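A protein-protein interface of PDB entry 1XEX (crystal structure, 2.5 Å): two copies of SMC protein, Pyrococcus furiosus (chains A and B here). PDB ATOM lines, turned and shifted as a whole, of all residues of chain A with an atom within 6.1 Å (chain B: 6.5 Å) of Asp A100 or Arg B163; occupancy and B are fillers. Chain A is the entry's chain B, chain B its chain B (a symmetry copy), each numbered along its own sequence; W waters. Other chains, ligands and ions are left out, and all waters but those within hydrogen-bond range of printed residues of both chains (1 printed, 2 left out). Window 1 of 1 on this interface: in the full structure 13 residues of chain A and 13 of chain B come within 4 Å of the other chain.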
ATOM      1  N   LEU A  98     -24.326 -20.496 -24.782  1.00  0.00           N
ATOM      2  CA  LEU A  98     -23.459 -19.467 -24.221  1.00  0.00           C
ATOM      3  C   LEU A  98     -22.066 -20.010 -23.907  1.00  0.00           C
ATOM      4  O   LEU A  98     -21.899 -21.206 -23.652  1.00  0.00           O
ATOM      5  CB  LEU A  98     -24.084 -18.896 -22.947  1.00  0.00           C
ATOM      6  CG  LEU A  98     -25.491 -18.297 -23.049  1.00  0.00           C
ATOM      7  CD1 LEU A  98     -25.984 -17.907 -21.662  1.00  0.00           C
ATOM      8  CD2 LEU A  98     -25.489 -17.096 -23.981  1.00  0.00           C
ATOM      9  N   ASP A  99     -21.065 -19.138 -23.979  1.00  0.00           N
ATOM     10  CA  ASP A  99     -19.692 -19.525 -23.673  1.00  0.00           C
ATOM     11  C   ASP A  99     -19.431 -19.403 -22.170  1.00  0.00           C
ATOM     12  O   ASP A  99     -20.261 -18.870 -21.434  1.00  0.00           O
ATOM     13  CB  ASP A  99     -18.690 -18.690 -24.485  1.00  0.00           C
ATOM     14  CG  ASP A  99     -18.676 -17.227 -24.086  1.00  0.00           C
ATOM     15  OD1 ASP A  99     -17.951 -16.871 -23.132  1.00  0.00           O
ATOM     16  OD2 ASP A  99     -19.368 -16.424 -24.746  1.00  0.00           O
ATOM     17  N   ASP A 100     -18.292 -19.923 -21.719  1.00  0.00           N
ATOM     18  CA  ASP A 100     -17.932 -19.901 -20.299  1.00  0.00           C
ATOM     19  C   ASP A 100     -18.055 -18.539 -19.619  1.00  0.00           C
ATOM     20  O   ASP A 100     -18.394 -18.462 -18.433  1.00  0.00           O
ATOM     21  CB  ASP A 100     -16.514 -20.441 -20.091  1.00  0.00           C
ATOM     22  CG  ASP A 100     -16.423 -21.942 -20.295  1.00  0.00           C
ATOM     23  OD1 ASP A 100     -15.405 -22.402 -20.851  1.00  0.00           O
ATOM     24  OD2 ASP A 100     -17.355 -22.669 -19.881  1.00  0.00           O
ATOM     25  N   ALA A 101     -17.726 -17.475 -20.343  1.00  0.00           N
ATOM     26  CA  ALA A 101     -17.814 -16.127 -19.792  1.00  0.00           C
ATOM     27  C   ALA A 101     -19.272 -15.715 -19.639  1.00  0.00           C
ATOM     28  O   ALA A 101     -19.667 -15.167 -18.606  1.00  0.00           O
ATOM     29  CB  ALA A 101     -17.070 -15.141 -20.683  1.00  0.00           C
ATOM     30  N   ASN A 102     -20.060 -15.959 -20.681  1.00  0.00           N
ATOM     31  CA  ASN A 102     -21.477 -15.619 -20.662  1.00  0.00           C
ATOM     32  C   ASN A 102     -22.275 -16.462 -19.672  1.00  0.00           C
ATOM     33  O   ASN A 102     -23.194 -15.954 -19.024  1.00  0.00           O
ATOM     34  CB  ASN A 102     -22.082 -15.720 -22.064  1.00  0.00           C
ATOM     35  CG  ASN A 102     -22.270 -14.361 -22.717  1.00  0.00           C
ATOM     36  OD1 ASN A 102     -21.717 -13.356 -22.263  1.00  0.00           O
ATOM     37  ND2 ASN A 102     -23.078 -14.316 -23.773  1.00  0.00           N
ATOM     38  N   VAL A 103     -21.926 -17.742 -19.552  1.00  0.00           N
ATOM     39  CA  VAL A 103     -22.600 -18.645 -18.621  1.00  0.00           C
ATOM     40  C   VAL A 103     -22.449 -18.087 -17.201  1.00  0.00           C
ATOM     41  O   VAL A 103     -23.400 -18.077 -16.406  1.00  0.00           O
ATOM     42  CB  VAL A 103     -21.970 -20.068 -18.629  1.00  0.00           C
ATOM     43  CG1 VAL A 103     -22.553 -20.879 -17.499  1.00  0.00           C
ATOM     44  CG2 VAL A 103     -22.195 -20.785 -19.971  1.00  0.00           C
ATOM     45  N   LYS A 104     -21.232 -17.647 -16.899  1.00  0.00           N
ATOM     46  CA  LYS A 104     -20.877 -17.093 -15.601  1.00  0.00           C
ATOM     47  C   LYS A 104     -21.702 -15.849 -15.304  1.00  0.00           C
ATOM     48  O   LYS A 104     -22.160 -15.655 -14.174  1.00  0.00           O
ATOM     49  CB  LYS A 104     -19.380 -16.753 -15.587  1.00  0.00           C
ATOM     50  CG  LYS A 104     -18.846 -16.200 -14.289  1.00  0.00           C
ATOM     51  CD  LYS A 104     -19.073 -17.164 -13.142  1.00  0.00           C
ATOM     52  CE  LYS A 104     -18.459 -16.628 -11.857  1.00  0.00           C
ATOM     53  NZ  LYS A 104     -19.444 -16.658 -10.723  1.00  0.00           N
ATOM     54  N   ARG A 105     -21.895 -15.005 -16.308  1.00  0.00           N
ATOM     55  CA  ARG A 105     -22.685 -13.813 -16.085  1.00  0.00           C
ATOM     56  C   ARG A 105     -24.138 -14.180 -15.763  1.00  0.00           C
ATOM     57  O   ARG A 105     -24.759 -13.584 -14.879  1.00  0.00           O
ATOM     58  CB  ARG A 105     -22.636 -12.894 -17.300  1.00  0.00           C
ATOM     59  CG  ARG A 105     -21.327 -12.143 -17.427  1.00  0.00           C
ATOM     60  CD  ARG A 105     -21.240 -11.403 -18.759  1.00  0.00           C
ATOM     61  NE  ARG A 105     -19.853 -11.071 -19.050  1.00  0.00           N
ATOM     62  CZ  ARG A 105     -19.189 -11.474 -20.128  1.00  0.00           C
ATOM     63  NH1 ARG A 105     -17.913 -11.119 -20.295  1.00  0.00           N
ATOM     64  NH2 ARG A 105     -19.797 -12.214 -21.048  1.00  0.00           N
ATOM     65  N   ARG A 125     -23.473 -27.604 -17.962  1.00  0.00           N
ATOM     66  CA  ARG A 125     -22.270 -26.783 -17.837  1.00  0.00           C
ATOM     67  C   ARG A 125     -21.760 -26.777 -16.398  1.00  0.00           C
ATOM     68  O   ARG A 125     -22.550 -26.796 -15.452  1.00  0.00           O
ATOM     69  CB  ARG A 125     -22.574 -25.349 -18.286  1.00  0.00           C
ATOM     70  CG  ARG A 125     -23.255 -25.247 -19.644  1.00  0.00           C
ATOM     71  CD  ARG A 125     -22.357 -25.766 -20.757  1.00  0.00           C
ATOM     72  NE  ARG A 125     -21.275 -24.832 -21.058  1.00  0.00           N
ATOM     73  CZ  ARG A 125     -21.365 -23.835 -21.932  1.00  0.00           C
ATOM     74  NH1 ARG A 125     -20.328 -23.037 -22.130  1.00  0.00           N
ATOM     75  NH2 ARG A 125     -22.480 -23.638 -22.620  1.00  0.00           N
ATOM     76  N   ASP A 126     -20.439 -26.755 -16.233  1.00  0.00           N
ATOM     77  CA  ASP A 126     -19.847 -26.745 -14.899  1.00  0.00           C
ATOM     78  C   ASP A 126     -19.842 -25.347 -14.281  1.00  0.00           C
ATOM     79  O   ASP A 126     -20.001 -25.202 -13.064  1.00  0.00           O
ATOM     80  CB  ASP A 126     -18.426 -27.323 -14.922  1.00  0.00           C
ATOM     81  CG  ASP A 126     -17.422 -26.400 -15.584  1.00  0.00           C
ATOM     82  OD1 ASP A 126     -16.617 -25.776 -14.848  1.00  0.00           O
ATOM     83  OD2 ASP A 126     -17.429 -26.317 -16.835  1.00  0.00           O
ATOM     84  N   VAL A 127     -19.681 -24.319 -15.113  1.00  0.00           N
ATOM     85  CA  VAL A 127     -19.663 -22.948 -14.612  1.00  0.00           C
ATOM     86  C   VAL A 127     -21.001 -22.595 -13.964  1.00  0.00           C
ATOM     87  O   VAL A 127     -21.040 -21.818 -13.013  1.00  0.00           O
ATOM     88  CB  VAL A 127     -19.346 -21.900 -15.721  1.00  0.00           C
ATOM     89  CG1 VAL A 127     -19.513 -20.477 -15.155  1.00  0.00           C
ATOM     90  CG2 VAL A 127     -17.902 -22.091 -16.236  1.00  0.00           C
ATOM     91  N   ARG A 163     -11.922 -35.251 -17.562  1.00  0.00           N
ATOM     92  CA  ARG A 163     -10.931 -34.497 -18.303  1.00  0.00           C
ATOM     93  C   ARG A 163      -9.507 -35.084 -18.277  1.00  0.00           C
ATOM     94  O   ARG A 163      -8.672 -34.733 -19.111  1.00  0.00           O
ATOM     95  CB  ARG A 163     -10.936 -33.031 -17.803  1.00  0.00           C
ATOM     96  CG  ARG A 163     -12.222 -32.261 -18.133  1.00  0.00           C
ATOM     97  CD  ARG A 163     -12.387 -31.018 -17.270  1.00  0.00           C
ATOM     98  NE  ARG A 163     -13.481 -30.163 -17.731  1.00  0.00           N
ATOM     99  CZ  ARG A 163     -14.784 -30.464 -17.675  1.00  0.00           C
ATOM    100  NH1 ARG A 163     -15.193 -31.619 -17.163  1.00  0.00           N
ATOM    101  NH2 ARG A 163     -15.690 -29.611 -18.151  1.00  0.00           N
ATOM    102  N   LEU B 124     -17.590 -24.320 -27.865  1.00  0.00           N
ATOM    103  CA  LEU B 124     -17.503 -23.438 -26.705  1.00  0.00           C
ATOM    104  C   LEU B 124     -17.141 -24.245 -25.458  1.00  0.00           C
ATOM    105  O   LEU B 124     -16.856 -23.678 -24.400  1.00  0.00           O
ATOM    106  CB  LEU B 124     -18.841 -22.723 -26.483  1.00  0.00           C
ATOM    107  CG  LEU B 124     -19.385 -21.831 -27.603  1.00  0.00           C
ATOM    108  CD1 LEU B 124     -20.776 -21.338 -27.231  1.00  0.00           C
ATOM    109  CD2 LEU B 124     -18.449 -20.655 -27.852  1.00  0.00           C
ATOM    110  N   ARG B 125     -17.185 -25.568 -25.590  1.00  0.00           N
ATOM    111  CA  ARG B 125     -16.878 -26.490 -24.498  1.00  0.00           C
ATOM    112  C   ARG B 125     -15.370 -26.630 -24.309  1.00  0.00           C
ATOM    113  O   ARG B 125     -14.612 -26.609 -25.282  1.00  0.00           O
ATOM    114  CB  ARG B 125     -17.495 -27.862 -24.791  1.00  0.00           C
ATOM    115  CG  ARG B 125     -18.970 -27.821 -25.171  1.00  0.00           C
ATOM    116  CD  ARG B 125     -19.824 -27.304 -24.024  1.00  0.00           C
ATOM    117  NE  ARG B 125     -19.967 -28.301 -22.966  1.00  0.00           N
ATOM    118  CZ  ARG B 125     -20.918 -29.229 -22.931  1.00  0.00           C
ATOM    119  NH1 ARG B 125     -20.959 -30.093 -21.930  1.00  0.00           N
ATOM    120  NH2 ARG B 125     -21.838 -29.290 -23.883  1.00  0.00           N
ATOM    121  N   ASP B 126     -14.936 -26.769 -23.059  1.00  0.00           N
ATOM    122  CA  ASP B 126     -13.512 -26.913 -22.768  1.00  0.00           C
ATOM    123  C   ASP B 126     -13.022 -28.345 -22.986  1.00  0.00           C
ATOM    124  O   ASP B 126     -11.880 -28.554 -23.410  1.00  0.00           O
ATOM    125  CB  ASP B 126     -13.192 -26.452 -21.340  1.00  0.00           C
ATOM    126  CG  ASP B 126     -13.702 -27.407 -20.280  1.00  0.00           C
ATOM    127  OD1 ASP B 126     -12.867 -28.140 -19.694  1.00  0.00           O
ATOM    128  OD2 ASP B 126     -14.930 -27.408 -20.024  1.00  0.00           O
ATOM    129  N   ILE B 158      -7.260 -18.799 -18.993  1.00  0.00           N
ATOM    130  CA  ILE B 158      -8.376 -17.914 -19.231  1.00  0.00           C
ATOM    131  C   ILE B 158      -9.654 -18.551 -18.658  1.00  0.00           C
ATOM    132  O   ILE B 158     -10.472 -17.873 -18.012  1.00  0.00           O
ATOM    133  CB  ILE B 158      -8.550 -17.661 -20.746  1.00  0.00           C
ATOM    134  CG1 ILE B 158      -7.467 -16.713 -21.247  1.00  0.00           C
ATOM    135  CG2 ILE B 158      -9.899 -17.040 -21.021  1.00  0.00           C
ATOM    136  CD1 ILE B 158      -7.336 -16.626 -22.776  1.00  0.00           C
ATOM    137  N   LEU B 159      -9.814 -19.854 -18.883  1.00  0.00           N
ATOM    138  CA  LEU B 159     -10.995 -20.541 -18.414  1.00  0.00           C
ATOM    139  C   LEU B 159     -11.037 -20.668 -16.902  1.00  0.00           C
ATOM    140  O   LEU B 159     -12.106 -20.580 -16.298  1.00  0.00           O
ATOM    141  CB  LEU B 159     -11.109 -21.918 -19.085  1.00  0.00           C
ATOM    142  CG  LEU B 159     -11.288 -21.857 -20.613  1.00  0.00           C
ATOM    143  CD1 LEU B 159     -11.354 -23.253 -21.189  1.00  0.00           C
ATOM    144  CD2 LEU B 159     -12.548 -21.081 -20.969  1.00  0.00           C
ATOM    145  N   GLU B 160      -9.882 -20.855 -16.277  1.00  0.00           N
ATOM    146  CA  GLU B 160      -9.856 -20.987 -14.828  1.00  0.00           C
ATOM    147  C   GLU B 160     -10.128 -19.648 -14.174  1.00  0.00           C
ATOM    148  O   GLU B 160     -10.680 -19.575 -13.070  1.00  0.00           O
ATOM    149  CB  GLU B 160      -8.513 -21.529 -14.380  1.00  0.00           C
ATOM    150  CG  GLU B 160      -8.191 -22.823 -15.087  1.00  0.00           C
ATOM    151  CD  GLU B 160      -6.789 -23.301 -14.823  1.00  0.00           C
ATOM    152  OE1 GLU B 160      -5.883 -22.444 -14.655  1.00  0.00           O
ATOM    153  OE2 GLU B 160      -6.580 -24.534 -14.804  1.00  0.00           O
ATOM    154  N   GLU B 161      -9.763 -18.583 -14.876  1.00  0.00           N
ATOM    155  CA  GLU B 161      -9.955 -17.247 -14.357  1.00  0.00           C
ATOM    156  C   GLU B 161     -11.441 -16.903 -14.378  1.00  0.00           C
ATOM    157  O   GLU B 161     -11.937 -16.253 -13.477  1.00  0.00           O
ATOM    158  CB  GLU B 161      -9.127 -16.249 -15.183  1.00  0.00           C
ATOM    159  CG  GLU B 161      -9.178 -14.797 -14.703  1.00  0.00           C
ATOM    160  CD  GLU B 161      -8.659 -14.612 -13.283  1.00  0.00           C
ATOM    161  OE1 GLU B 161      -7.675 -15.278 -12.896  1.00  0.00           O
ATOM    162  OE2 GLU B 161      -9.225 -13.783 -12.550  1.00  0.00           O
ATOM    163  N   ILE B 162     -12.150 -17.353 -15.403  1.00  0.00           N
ATOM    164  CA  ILE B 162     -13.589 -17.099 -15.512  1.00  0.00           C
ATOM    165  C   ILE B 162     -14.299 -17.774 -14.329  1.00  0.00           C
ATOM    166  O   ILE B 162     -15.286 -17.270 -13.809  1.00  0.00           O
ATOM    167  CB  ILE B 162     -14.182 -17.697 -16.839  1.00  0.00           C
ATOM    168  CG1 ILE B 162     -13.785 -16.844 -18.059  1.00  0.00           C
ATOM    169  CG2 ILE B 162     -15.697 -17.831 -16.720  1.00  0.00           C
ATOM    170  N   ARG B 163     -13.770 -18.918 -13.921  1.00  0.00           N
ATOM    171  CA  ARG B 163     -14.346 -19.700 -12.846  1.00  0.00           C
ATOM    172  C   ARG B 163     -13.977 -19.232 -11.426  1.00  0.00           C
ATOM    173  O   ARG B 163     -14.643 -19.595 -10.456  1.00  0.00           O
ATOM    174  CB  ARG B 163     -13.978 -21.189 -13.053  1.00  0.00           C
ATOM    175  CG  ARG B 163     -14.630 -21.831 -14.286  1.00  0.00           C
ATOM    176  CD  ARG B 163     -13.924 -23.109 -14.712  1.00  0.00           C
ATOM    177  NE  ARG B 163     -14.669 -23.842 -15.736  1.00  0.00           N
ATOM    178  CZ  ARG B 163     -14.862 -23.441 -16.998  1.00  0.00           C
ATOM    179  NH1 ARG B 163     -14.356 -22.293 -17.431  1.00  0.00           N
ATOM    180  NH2 ARG B 163     -15.583 -24.186 -17.835  1.00  0.00           N
ATOM    181  N   LYS B 164     -12.923 -18.436 -11.288  1.00  0.00           N
ATOM    182  CA  LYS B 164     -12.551 -17.947  -9.963  1.00  0.00           C
ATOM    183  C   LYS B 164     -13.627 -16.956  -9.500  1.00  0.00           C
ATOM    184  O   LYS B 164     -14.373 -16.416 -10.312  1.00  0.00           O
ATOM    185  CB  LYS B 164     -11.187 -17.247 -10.012  1.00  0.00           C
ATOM    186  N   LYS B 165     -13.728 -16.742  -8.195  1.00  0.00           N
ATOM    187  CA  LYS B 165     -14.704 -15.797  -7.650  1.00  0.00           C
ATOM    188  C   LYS B 165     -14.027 -14.429  -7.558  1.00  0.00           C
ATOM    189  O   LYS B 165     -13.197 -14.205  -6.667  1.00  0.00           O
ATOM    190  CB  LYS B 165     -15.154 -16.235  -6.250  1.00  0.00           C
ATOM    191  CG  LYS B 165     -15.853 -15.137  -5.442  1.00  0.00           C
ATOM    192  CD  LYS B 165     -15.964 -15.511  -3.959  1.00  0.00           C
ATOM    193  CE  LYS B 165     -16.591 -14.380  -3.139  1.00  0.00           C
ATOM    194  NZ  LYS B 165     -16.705 -14.709  -1.682  1.00  0.00           N
ATOM    195  N   GLN B 166     -14.369 -13.521  -8.472  1.00  0.00           N
ATOM    196  CA  GLN B 166     -13.771 -12.184  -8.473  1.00  0.00           C
ATOM    197  C   GLN B 166     -14.606 -11.137  -7.723  1.00  0.00           C
ATOM    198  O   GLN B 166     -14.730 -11.188  -6.490  1.00  0.00           O
ATOM    199  CB  GLN B 166     -13.524 -11.704  -9.911  1.00  0.00           C
ATOM    200  CG  GLN B 166     -12.228 -12.209 -10.553  1.00  0.00           C
ATOM    201  CD  GLN B 166     -12.318 -13.640 -11.082  1.00  0.00           C
ATOM    202  OE1 GLN B 166     -13.165 -13.955 -11.931  1.00  0.00           O
ATOM    203  NE2 GLN B 166     -11.432 -14.509 -10.592  1.00  0.00           N
HETATM  204  O   HOH W   1     -16.356 -25.182 -20.948  1.00  0.00           O
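Of the 12 printed residues of chain A, 7 touch a printed residue of chain B.
Hydrophobic or aromatic side chains of chain B that line the printed part of chain A: Leu B124, Leu B159 and Ile B162.
Along chain B the printed residues that touch a printed residue of chain A span positions 124 to 163.
Water W1 lies within hydrogen-bond range of the side-chain carboxylate (OD2) of Asp B126 (2.8 Å), the side-chain carboxylate (OD2) of Asp A100 (2.9 Å) and the guanidinium group (NH2) of Arg B163 (3.4 Å).
The side-chain carboxylate (OD2) of Asp A100 is in salt-bridge range of the guanidinium group (NH2) of Arg B163 (3.1 Å).
OD1 of Asp A126 lies within salt-bridge range of NE of Arg B163.
The side-chain carboxylate (OD1) of Asp B126 lies within salt-bridge range of the guanidinium group (NE) of Arg A163, at 2.9 Å.
Asp A126 touches Arg B163, and with the chains exchanged Arg A163 touches Asp B126.
Positions printed for both chains: 125, 126 and 163.
Of the 9 pairs that touch across the chains among the printed residues, 2 have their exchanged pair printed and touching as well.
Among the printed residues, merely in contact across the chains: Leu A98 with Leu B124 (3.8 Å), Asp A99 with Leu B124 (3.9 Å), Asp A100 with Leu B159 (3.1 Å), Asp A100 with Ile B162 (3.3 Å), Lys A104 with Ile B162 (3.7 Å) and Val A127 with Arg B163 (3.4 Å).
Arg B163 touches just these residues of chain A: Asp A100, Asp A126 and Val A127.
Of the printed residues of chain A, Ile B162 touches Asp A100 and Lys A104.
Of the printed residues of chain A, Asp B126 touches Arg A163.
Printed residues of chain A within 4 Å of Leu B159: Asp A100.
Printed residues of chain B within 4 Å of Asp A126: Arg B163 (2.9 Å).
Lys B165 touches none of the printed residues of chain A.
The nearest residue of chain B that does not touch Asp A100 is Leu B124 (4.04 Å).
The nearest residue of chain A that does not touch Arg B163 is Lys A104 (5.0 Å).
NH2 of Arg A125 is in hydrogen-bond range of O of Leu A98 (2.7 Å).
The side-chain carboxylate (OD1) of Asp A99 lies within hydrogen-bond range of the backbone NH (N) of Ala A101, 2.9 Å away.
OD2 of Asp A100 is in salt-bridge range of NH1 of Arg A125 (3.7 Å).
OD2 of Asp A126 lies within salt-bridge range of NH2 of Arg A163 (3.95 Å).
The guanidinium group (NH2) of Arg B163 is in salt-bridge range of the side-chain carboxylate (OD2) of Asp B126, at 3.9 Å.
The guanidinium group (NH1) of Arg B163 sits at hydrogen-bond distance from the backbone carbonyl oxygen (O) of Leu B159, 3.0 Å away.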
